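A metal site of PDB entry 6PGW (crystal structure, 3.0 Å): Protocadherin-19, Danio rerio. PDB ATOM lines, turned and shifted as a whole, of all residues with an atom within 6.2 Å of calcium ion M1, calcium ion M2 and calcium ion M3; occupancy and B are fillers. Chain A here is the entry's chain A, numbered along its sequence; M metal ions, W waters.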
ATOM      1  N   GLU A 230      10.609  18.564   1.509  1.00  0.00           N
ATOM      2  CA  GLU A 230      10.068  17.938   0.323  1.00  0.00           C
ATOM      3  C   GLU A 230      10.936  18.312  -0.899  1.00  0.00           C
ATOM      4  O   GLU A 230      11.636  19.329  -0.886  1.00  0.00           O
ATOM      5  CB  GLU A 230       8.599  18.397   0.205  1.00  0.00           C
ATOM      6  CG  GLU A 230       7.999  18.394  -1.150  1.00  0.00           C
ATOM      7  CD  GLU A 230       6.509  18.636  -1.115  1.00  0.00           C
ATOM      8  OE1 GLU A 230       6.008  19.543  -0.387  1.00  0.00           O
ATOM      9  OE2 GLU A 230       5.839  17.935  -1.839  1.00  0.00           O
ATOM     10  N   ASN A 231      10.948  17.439  -1.909  1.00  0.00           N
ATOM     11  CA  ASN A 231      11.794  17.610  -3.119  1.00  0.00           C
ATOM     12  C   ASN A 231      13.324  17.637  -2.828  1.00  0.00           C
ATOM     13  O   ASN A 231      14.077  18.345  -3.503  1.00  0.00           O
ATOM     14  CB  ASN A 231      11.395  18.879  -3.898  1.00  0.00           C
ATOM     15  CG  ASN A 231       9.917  18.937  -4.195  1.00  0.00           C
ATOM     16  OD1 ASN A 231       9.278  17.916  -4.344  1.00  0.00           O
ATOM     17  ND2 ASN A 231       9.376  20.143  -4.272  1.00  0.00           N
ATOM     18  N   PHE A 286      11.569  12.861  -1.968  1.00  0.00           N
ATOM     19  CA  PHE A 286      10.319  12.793  -1.187  1.00  0.00           C
ATOM     20  C   PHE A 286       9.292  13.887  -1.587  1.00  0.00           C
ATOM     21  O   PHE A 286       9.651  14.963  -2.075  1.00  0.00           O
ATOM     22  CB  PHE A 286      10.619  12.888   0.319  1.00  0.00           C
ATOM     23  CG  PHE A 286      11.555  11.817   0.839  1.00  0.00           C
ATOM     24  CD1 PHE A 286      11.562  10.529   0.326  1.00  0.00           C
ATOM     25  CD2 PHE A 286      12.396  12.094   1.915  1.00  0.00           C
ATOM     26  CE1 PHE A 286      12.417   9.568   0.835  1.00  0.00           C
ATOM     27  CE2 PHE A 286      13.254  11.127   2.416  1.00  0.00           C
ATOM     28  CZ  PHE A 286      13.262   9.871   1.876  1.00  0.00           C
ATOM     29  N   ASN A 287       8.016  13.599  -1.342  1.00  0.00           N
ATOM     30  CA  ASN A 287       6.894  14.442  -1.753  1.00  0.00           C
ATOM     31  C   ASN A 287       5.768  14.377  -0.724  1.00  0.00           C
ATOM     32  O   ASN A 287       5.007  13.434  -0.692  1.00  0.00           O
ATOM     33  CB  ASN A 287       6.363  13.982  -3.096  1.00  0.00           C
ATOM     34  CG  ASN A 287       5.127  14.766  -3.528  1.00  0.00           C
ATOM     35  OD1 ASN A 287       4.791  15.814  -2.957  1.00  0.00           O
ATOM     36  ND2 ASN A 287       4.463  14.250  -4.544  1.00  0.00           N
ATOM     37  N   HIS A 288       5.677  15.429   0.085  1.00  0.00           N
ATOM     38  CA  HIS A 288       4.661  15.607   1.126  1.00  0.00           C
ATOM     39  C   HIS A 288       3.212  15.313   0.699  1.00  0.00           C
ATOM     40  O   HIS A 288       2.348  15.014   1.512  1.00  0.00           O
ATOM     41  CB  HIS A 288       4.758  17.041   1.605  1.00  0.00           C
ATOM     42  CG  HIS A 288       3.770  17.401   2.655  1.00  0.00           C
ATOM     43  ND1 HIS A 288       4.124  17.519   3.982  1.00  0.00           N
ATOM     44  CD2 HIS A 288       2.456  17.721   2.583  1.00  0.00           C
ATOM     45  CE1 HIS A 288       3.061  17.866   4.690  1.00  0.00           C
ATOM     46  NE2 HIS A 288       2.034  17.988   3.865  1.00  0.00           N
ATOM     47  N   GLU A 289       2.949  15.422  -0.582  1.00  0.00           N
ATOM     48  CA  GLU A 289       1.651  15.132  -1.093  1.00  0.00           C
ATOM     49  C   GLU A 289       1.466  13.584  -1.314  1.00  0.00           C
ATOM     50  O   GLU A 289       0.360  13.096  -1.578  1.00  0.00           O
ATOM     51  CB  GLU A 289       1.470  15.943  -2.371  1.00  0.00           C
ATOM     52  CG  GLU A 289       1.221  17.445  -2.117  1.00  0.00           C
ATOM     53  CD  GLU A 289       2.420  18.218  -1.571  1.00  0.00           C
ATOM     54  OE1 GLU A 289       2.301  19.026  -0.616  1.00  0.00           O
ATOM     55  OE2 GLU A 289       3.511  18.033  -2.093  1.00  0.00           O
ATOM     56  N   LEU A 319       8.366  17.629   5.439  1.00  0.00           N
ATOM     57  CA  LEU A 319       7.859  18.969   5.604  1.00  0.00           C
ATOM     58  C   LEU A 319       7.322  19.551   4.290  1.00  0.00           C
ATOM     59  O   LEU A 319       7.779  19.202   3.215  1.00  0.00           O
ATOM     60  CB  LEU A 319       8.958  19.851   6.115  1.00  0.00           C
ATOM     61  CG  LEU A 319       9.652  19.392   7.400  1.00  0.00           C
ATOM     62  CD1 LEU A 319      10.885  20.246   7.632  1.00  0.00           C
ATOM     63  CD2 LEU A 319       8.724  19.456   8.602  1.00  0.00           C
ATOM     64  N   ASP A 320       6.358  20.447   4.401  1.00  0.00           N
ATOM     65  CA  ASP A 320       5.640  20.974   3.244  1.00  0.00           C
ATOM     66  C   ASP A 320       6.412  22.133   2.665  1.00  0.00           C
ATOM     67  O   ASP A 320       6.832  23.047   3.400  1.00  0.00           O
ATOM     68  CB  ASP A 320       4.243  21.424   3.673  1.00  0.00           C
ATOM     69  CG  ASP A 320       3.372  21.929   2.500  1.00  0.00           C
ATOM     70  OD1 ASP A 320       3.429  21.362   1.356  1.00  0.00           O
ATOM     71  OD2 ASP A 320       2.614  22.895   2.755  1.00  0.00           O
ATOM     72  N   VAL A 321       6.594  22.091   1.359  1.00  0.00           N
ATOM     73  CA  VAL A 321       6.984  23.264   0.600  1.00  0.00           C
ATOM     74  C   VAL A 321       5.941  23.561  -0.477  1.00  0.00           C
ATOM     75  O   VAL A 321       5.215  22.644  -0.937  1.00  0.00           O
ATOM     76  CB  VAL A 321       8.403  23.130  -0.001  1.00  0.00           C
ATOM     77  CG1 VAL A 321       9.392  22.685   1.065  1.00  0.00           C
ATOM     78  CG2 VAL A 321       8.414  22.155  -1.178  1.00  0.00           C
ATOM     79  N   ASN A 322       5.869  24.849  -0.831  1.00  0.00           N
ATOM     80  CA  ASN A 322       4.842  25.381  -1.706  1.00  0.00           C
ATOM     81  C   ASN A 322       5.230  25.059  -3.142  1.00  0.00           C
ATOM     82  O   ASN A 322       5.597  25.942  -3.914  1.00  0.00           O
ATOM     83  CB  ASN A 322       4.674  26.911  -1.506  1.00  0.00           C
ATOM     84  CG  ASN A 322       3.449  27.472  -2.222  1.00  0.00           C
ATOM     85  OD1 ASN A 322       2.520  26.713  -2.584  1.00  0.00           O
ATOM     86  ND2 ASN A 322       3.432  28.801  -2.442  1.00  0.00           N
ATOM     87  N   ASP A 323       5.112  23.787  -3.490  1.00  0.00           N
ATOM     88  CA  ASP A 323       5.622  23.242  -4.737  1.00  0.00           C
ATOM     89  C   ASP A 323       4.487  22.804  -5.606  1.00  0.00           C
ATOM     90  O   ASP A 323       4.642  22.004  -6.521  1.00  0.00           O
ATOM     91  CB  ASP A 323       6.554  22.066  -4.441  1.00  0.00           C
ATOM     92  CG  ASP A 323       5.851  20.853  -3.779  1.00  0.00           C
ATOM     93  OD1 ASP A 323       4.845  21.002  -2.994  1.00  0.00           O
ATOM     94  OD2 ASP A 323       6.344  19.739  -4.023  1.00  0.00           O
ATOM     95  N   ASN A 324       3.319  23.340  -5.293  1.00  0.00           N
ATOM     96  CA  ASN A 324       2.149  23.158  -6.093  1.00  0.00           C
ATOM     97  C   ASN A 324       1.510  24.505  -6.247  1.00  0.00           C
ATOM     98  O   ASN A 324       1.018  25.141  -5.215  1.00  0.00           O
ATOM     99  CB  ASN A 324       1.149  22.240  -5.429  1.00  0.00           C
ATOM    100  CG  ASN A 324       1.534  20.808  -5.504  1.00  0.00           C
ATOM    101  OD1 ASN A 324       1.498  20.200  -6.559  1.00  0.00           O
ATOM    102  ND2 ASN A 324       1.850  20.241  -4.346  1.00  0.00           N
ATOM    103  N   THR A 325       1.576  24.978  -7.497  1.00  0.00           N
ATOM    104  CA  THR A 325       0.744  26.065  -8.020  1.00  0.00           C
ATOM    105  C   THR A 325      -0.708  25.596  -8.033  1.00  0.00           C
ATOM    106  O   THR A 325      -0.988  24.476  -8.427  1.00  0.00           O
ATOM    107  CB  THR A 325       1.123  26.412  -9.484  1.00  0.00           C
ATOM    108  OG1 THR A 325       1.302  25.191 -10.212  1.00  0.00           O
ATOM    109  CG2 THR A 325       2.391  27.224  -9.584  1.00  0.00           C
ATOM    110  N   PRO A 326      -1.639  26.494  -7.649  1.00  0.00           N
ATOM    111  CA  PRO A 326      -3.086  26.190  -7.578  1.00  0.00           C
ATOM    112  C   PRO A 326      -3.706  25.807  -8.919  1.00  0.00           C
ATOM    113  O   PRO A 326      -3.141  26.117  -9.954  1.00  0.00           O
ATOM    114  CB  PRO A 326      -3.697  27.510  -7.118  1.00  0.00           C
ATOM    115  CG  PRO A 326      -2.594  28.248  -6.462  1.00  0.00           C
ATOM    116  CD  PRO A 326      -1.329  27.830  -7.116  1.00  0.00           C
ATOM    117  N   ASP A 359      -5.564  23.425  -4.346  1.00  0.00           N
ATOM    118  CA  ASP A 359      -4.068  23.505  -4.164  1.00  0.00           C
ATOM    119  C   ASP A 359      -3.743  22.375  -3.189  1.00  0.00           C
ATOM    120  O   ASP A 359      -4.438  22.192  -2.191  1.00  0.00           O
ATOM    121  CB  ASP A 359      -3.646  24.869  -3.569  1.00  0.00           C
ATOM    122  CG  ASP A 359      -2.109  25.090  -3.520  1.00  0.00           C
ATOM    123  OD1 ASP A 359      -1.373  24.269  -2.998  1.00  0.00           O
ATOM    124  OD2 ASP A 359      -1.667  26.149  -3.909  1.00  0.00           O
ATOM    125  N   TYR A 360      -2.719  21.590  -3.482  1.00  0.00           N
ATOM    126  CA  TYR A 360      -2.467  20.379  -2.701  1.00  0.00           C
ATOM    127  C   TYR A 360      -1.657  20.567  -1.490  1.00  0.00           C
ATOM    128  O   TYR A 360      -1.796  19.811  -0.513  1.00  0.00           O
ATOM    129  CB  TYR A 360      -1.845  19.315  -3.585  1.00  0.00           C
ATOM    130  CG  TYR A 360      -2.691  19.064  -4.817  1.00  0.00           C
ATOM    131  CD1 TYR A 360      -4.078  18.888  -4.715  1.00  0.00           C
ATOM    132  CD2 TYR A 360      -2.127  19.093  -6.075  1.00  0.00           C
ATOM    133  CE1 TYR A 360      -4.856  18.677  -5.832  1.00  0.00           C
ATOM    134  CE2 TYR A 360      -2.901  18.899  -7.205  1.00  0.00           C
ATOM    135  CZ  TYR A 360      -4.262  18.681  -7.066  1.00  0.00           C
ATOM    136  OH  TYR A 360      -5.016  18.488  -8.173  1.00  0.00           O
ATOM    137  N   ASP A 361      -0.854  21.599  -1.465  1.00  0.00           N
ATOM    138  CA  ASP A 361      -0.025  21.817  -0.343  1.00  0.00           C
ATOM    139  C   ASP A 361      -0.890  21.972   0.912  1.00  0.00           C
ATOM    140  O   ASP A 361      -2.116  22.129   0.815  1.00  0.00           O
ATOM    141  CB  ASP A 361       0.850  23.018  -0.548  1.00  0.00           C
ATOM    142  CG  ASP A 361       1.718  22.904  -1.794  1.00  0.00           C
ATOM    143  OD1 ASP A 361       2.325  21.802  -2.019  1.00  0.00           O
ATOM    144  OD2 ASP A 361       1.809  23.951  -2.523  1.00  0.00           O
ATOM    145  N   GLU A 362      -0.278  21.854   2.065  1.00  0.00           N
ATOM    146  CA  GLU A 362      -1.013  21.989   3.318  1.00  0.00           C
ATOM    147  C   GLU A 362      -0.669  23.326   3.939  1.00  0.00           C
ATOM    148  O   GLU A 362       0.390  23.880   3.688  1.00  0.00           O
ATOM    149  CB  GLU A 362      -0.668  20.852   4.252  1.00  0.00           C
ATOM    150  CG  GLU A 362      -1.227  20.990   5.680  1.00  0.00           C
ATOM    151  CD  GLU A 362      -0.176  20.750   6.752  1.00  0.00           C
ATOM    152  OE1 GLU A 362      -0.509  20.909   7.961  1.00  0.00           O
ATOM    153  OE2 GLU A 362       0.972  20.367   6.407  1.00  0.00           O
ATOM    154  N   GLU A 364      -0.675  27.282   4.985  1.00  0.00           N
ATOM    155  CA  GLU A 364      -0.649  28.541   4.277  1.00  0.00           C
ATOM    156  C   GLU A 364      -0.359  28.298   2.818  1.00  0.00           C
ATOM    157  O   GLU A 364      -0.943  28.919   1.949  1.00  0.00           O
ATOM    158  CB  GLU A 364       0.401  29.464   4.870  1.00  0.00           C
ATOM    159  CG  GLU A 364       0.128  29.900   6.294  1.00  0.00           C
ATOM    160  CD  GLU A 364      -0.923  30.996   6.381  1.00  0.00           C
ATOM    161  OE1 GLU A 364      -0.582  32.175   6.122  1.00  0.00           O
ATOM    162  OE2 GLU A 364      -2.090  30.665   6.707  1.00  0.00           O
ATOM    163  N   ASN A 365       0.507  27.335   2.574  1.00  0.00           N
ATOM    164  CA  ASN A 365       0.879  26.944   1.261  1.00  0.00           C
ATOM    165  C   ASN A 365      -0.291  26.515   0.467  1.00  0.00           C
ATOM    166  O   ASN A 365      -0.261  26.530  -0.795  1.00  0.00           O
ATOM    167  CB  ASN A 365       1.811  25.781   1.316  1.00  0.00           C
ATOM    168  CG  ASN A 365       3.158  26.140   1.891  1.00  0.00           C
ATOM    169  OD1 ASN A 365       4.180  25.800   1.328  1.00  0.00           O
ATOM    170  ND2 ASN A 365       3.161  26.827   3.017  1.00  0.00           N
ATOM    171  N   GLY A 366      -1.293  26.014   1.159  1.00  0.00           N
ATOM    172  CA  GLY A 366      -2.461  25.518   0.512  1.00  0.00           C
ATOM    173  C   GLY A 366      -3.670  26.388   0.548  1.00  0.00           C
ATOM    174  O   GLY A 366      -4.729  25.981   0.050  1.00  0.00           O
ATOM    175  N   ARG A 367      -3.545  27.581   1.142  1.00  0.00           N
ATOM    176  CA  ARG A 367      -4.719  28.453   1.352  1.00  0.00           C
ATOM    177  C   ARG A 367      -4.956  29.349   0.143  1.00  0.00           C
ATOM    178  O   ARG A 367      -3.996  29.933  -0.416  1.00  0.00           O
ATOM    179  CB  ARG A 367      -4.542  29.312   2.587  1.00  0.00           C
ATOM    180  CG  ARG A 367      -5.850  29.634   3.319  1.00  0.00           C
ATOM    181  CD  ARG A 367      -5.611  30.567   4.492  1.00  0.00           C
ATOM    182  NE  ARG A 367      -5.441  31.969   4.088  1.00  0.00           N
ATOM    183  CZ  ARG A 367      -4.388  32.720   4.362  1.00  0.00           C
ATOM    184  NH1 ARG A 367      -4.370  33.986   3.988  1.00  0.00           N
ATOM    185  NH2 ARG A 367      -3.345  32.232   5.034  1.00  0.00           N
ATOM    186  N   ASP A 411      -2.181  31.659  -3.707  1.00  0.00           N
ATOM    187  CA  ASP A 411      -2.061  30.999  -2.395  1.00  0.00           C
ATOM    188  C   ASP A 411      -1.193  31.807  -1.405  1.00  0.00           C
ATOM    189  O   ASP A 411      -0.869  32.978  -1.680  1.00  0.00           O
ATOM    190  CB  ASP A 411      -1.604  29.521  -2.535  1.00  0.00           C
ATOM    191  CG  ASP A 411      -0.122  29.365  -2.938  1.00  0.00           C
ATOM    192  OD1 ASP A 411       0.582  30.397  -3.109  1.00  0.00           O
ATOM    193  OD2 ASP A 411       0.325  28.161  -3.098  1.00  0.00           O
ATOM    194  N   LEU A 417       2.326  31.030  -5.001  1.00  0.00           N
ATOM    195  CA  LEU A 417       2.007  30.594  -6.357  1.00  0.00           C
ATOM    196  C   LEU A 417       0.565  31.001  -6.702  1.00  0.00           C
ATOM    197  O   LEU A 417      -0.154  31.495  -5.819  1.00  0.00           O
ATOM    198  CB  LEU A 417       2.243  29.080  -6.549  1.00  0.00           C
ATOM    199  CG  LEU A 417       3.695  28.601  -6.866  1.00  0.00           C
ATOM    200  CD1 LEU A 417       4.368  29.446  -7.950  1.00  0.00           C
ATOM    201  CD2 LEU A 417       4.561  28.605  -5.620  1.00  0.00           C
HETATM  202 CA    CA M   1       3.978  20.647  -0.811  1.00  0.00          CA
HETATM  203 CA    CA M   2       4.899  17.943  -3.925  1.00  0.00          CA
HETATM  204 CA    CA M   3       0.436  25.788  -2.990  1.00  0.00          CA
HETATM  205  O   HOH W   1       3.304  18.174  -5.586  1.00  0.00           O
HETATM  206  O   HOH W   2       6.947  17.015  -4.426  1.00  0.00           O
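The side-chain carboxylate (OE2) of Glu 230 lies close to the backbone NH (N) of His 288, 3.2 Å away. The backbone carbonyl oxygen (O) of Leu 319 sits close to the backbone NH (N) of Glu 230, at 3.4 Å. OD1 of Asp 323 lies close to ND2 of Asn 324 (3.4 Å). The side-chain carboxylate (OD2) of Asp 323 lies close to the side-chain amide nitrogen (ND2) of Asn 231 (3.1 Å). The side-chain carboxylate (OD2) of Asp 320 lies within hydrogen-bond range of the backbone NH (N) of Glu 362 (3.2 Å). The backbone NH (N) of Leu 417 sits at hydrogen-bond distance from the side-chain carboxylate (OD1) of Asp 411 (2.6 Å).
Along chain A the residues within 4 Å of calcium ion M1 span positions 230 to 361. The nearest printed residue that does not touch calcium ion M1 is Asn 324 (4.1 Å).
Five residues have an atom within 4 Å of calcium ion M2: Glu 230, Asn 287, Glu 289, Asp 323 and Asn 324.
Six residues have an atom within 4 Å of calcium ion M3: Asn 322, Asn 324, Asp 359, Asp 361, Asn 365 and Asp 411. The nearest printed residue that does not touch calcium ion M3 is Gly 366 (4.5 Å).
Calcium ion M1 is bound by OE1 of Glu 289, OD1 of Asp 320, OE1 of Glu 230, OD1 of Asp 361, O of Val 321 and OD1 of Asp 323. Slightly farther from calcium ion M1 lies OE2 of Glu 289 (2.9 Å).
OE2 of Glu 230 is bound to calcium ion M2, at 2.3 Å. OE2 of Glu 289 binds calcium ion M2. Calcium ion M2 is bound by water W2, at 2.3 Å. Calcium ion M2 is bound by OD2 of Asp 323, 2.3 Å away. Water W1 is bound to calcium ion M2 (2.3 Å). The side-chain amide oxygen (OD1) of Asn 287 is bound to calcium ion M2 (2.3 Å). Calcium ion M2 has six donor atoms within binding distance.
Calcium ion M3 is bound by OD1 of Asn 322, 2.3 Å away. Calcium ion M3 is bound by OD2 of Asp 359, 2.3 Å away. OD2 of Asp 361 binds calcium ion M3 (2.3 Å). The side-chain carboxylate (OD1) of Asp 359 binds calcium ion M3. Calcium ion M3 is bound by the side-chain carboxylate (OD2) of Asp 411 (2.4 Å). O of Asn 324 is bound to calcium ion M3 (2.4 Å). O of Asn 365 is bound to calcium ion M3, 2.4 Å away. Calcium ion M3 has seven donor atoms within binding distance.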
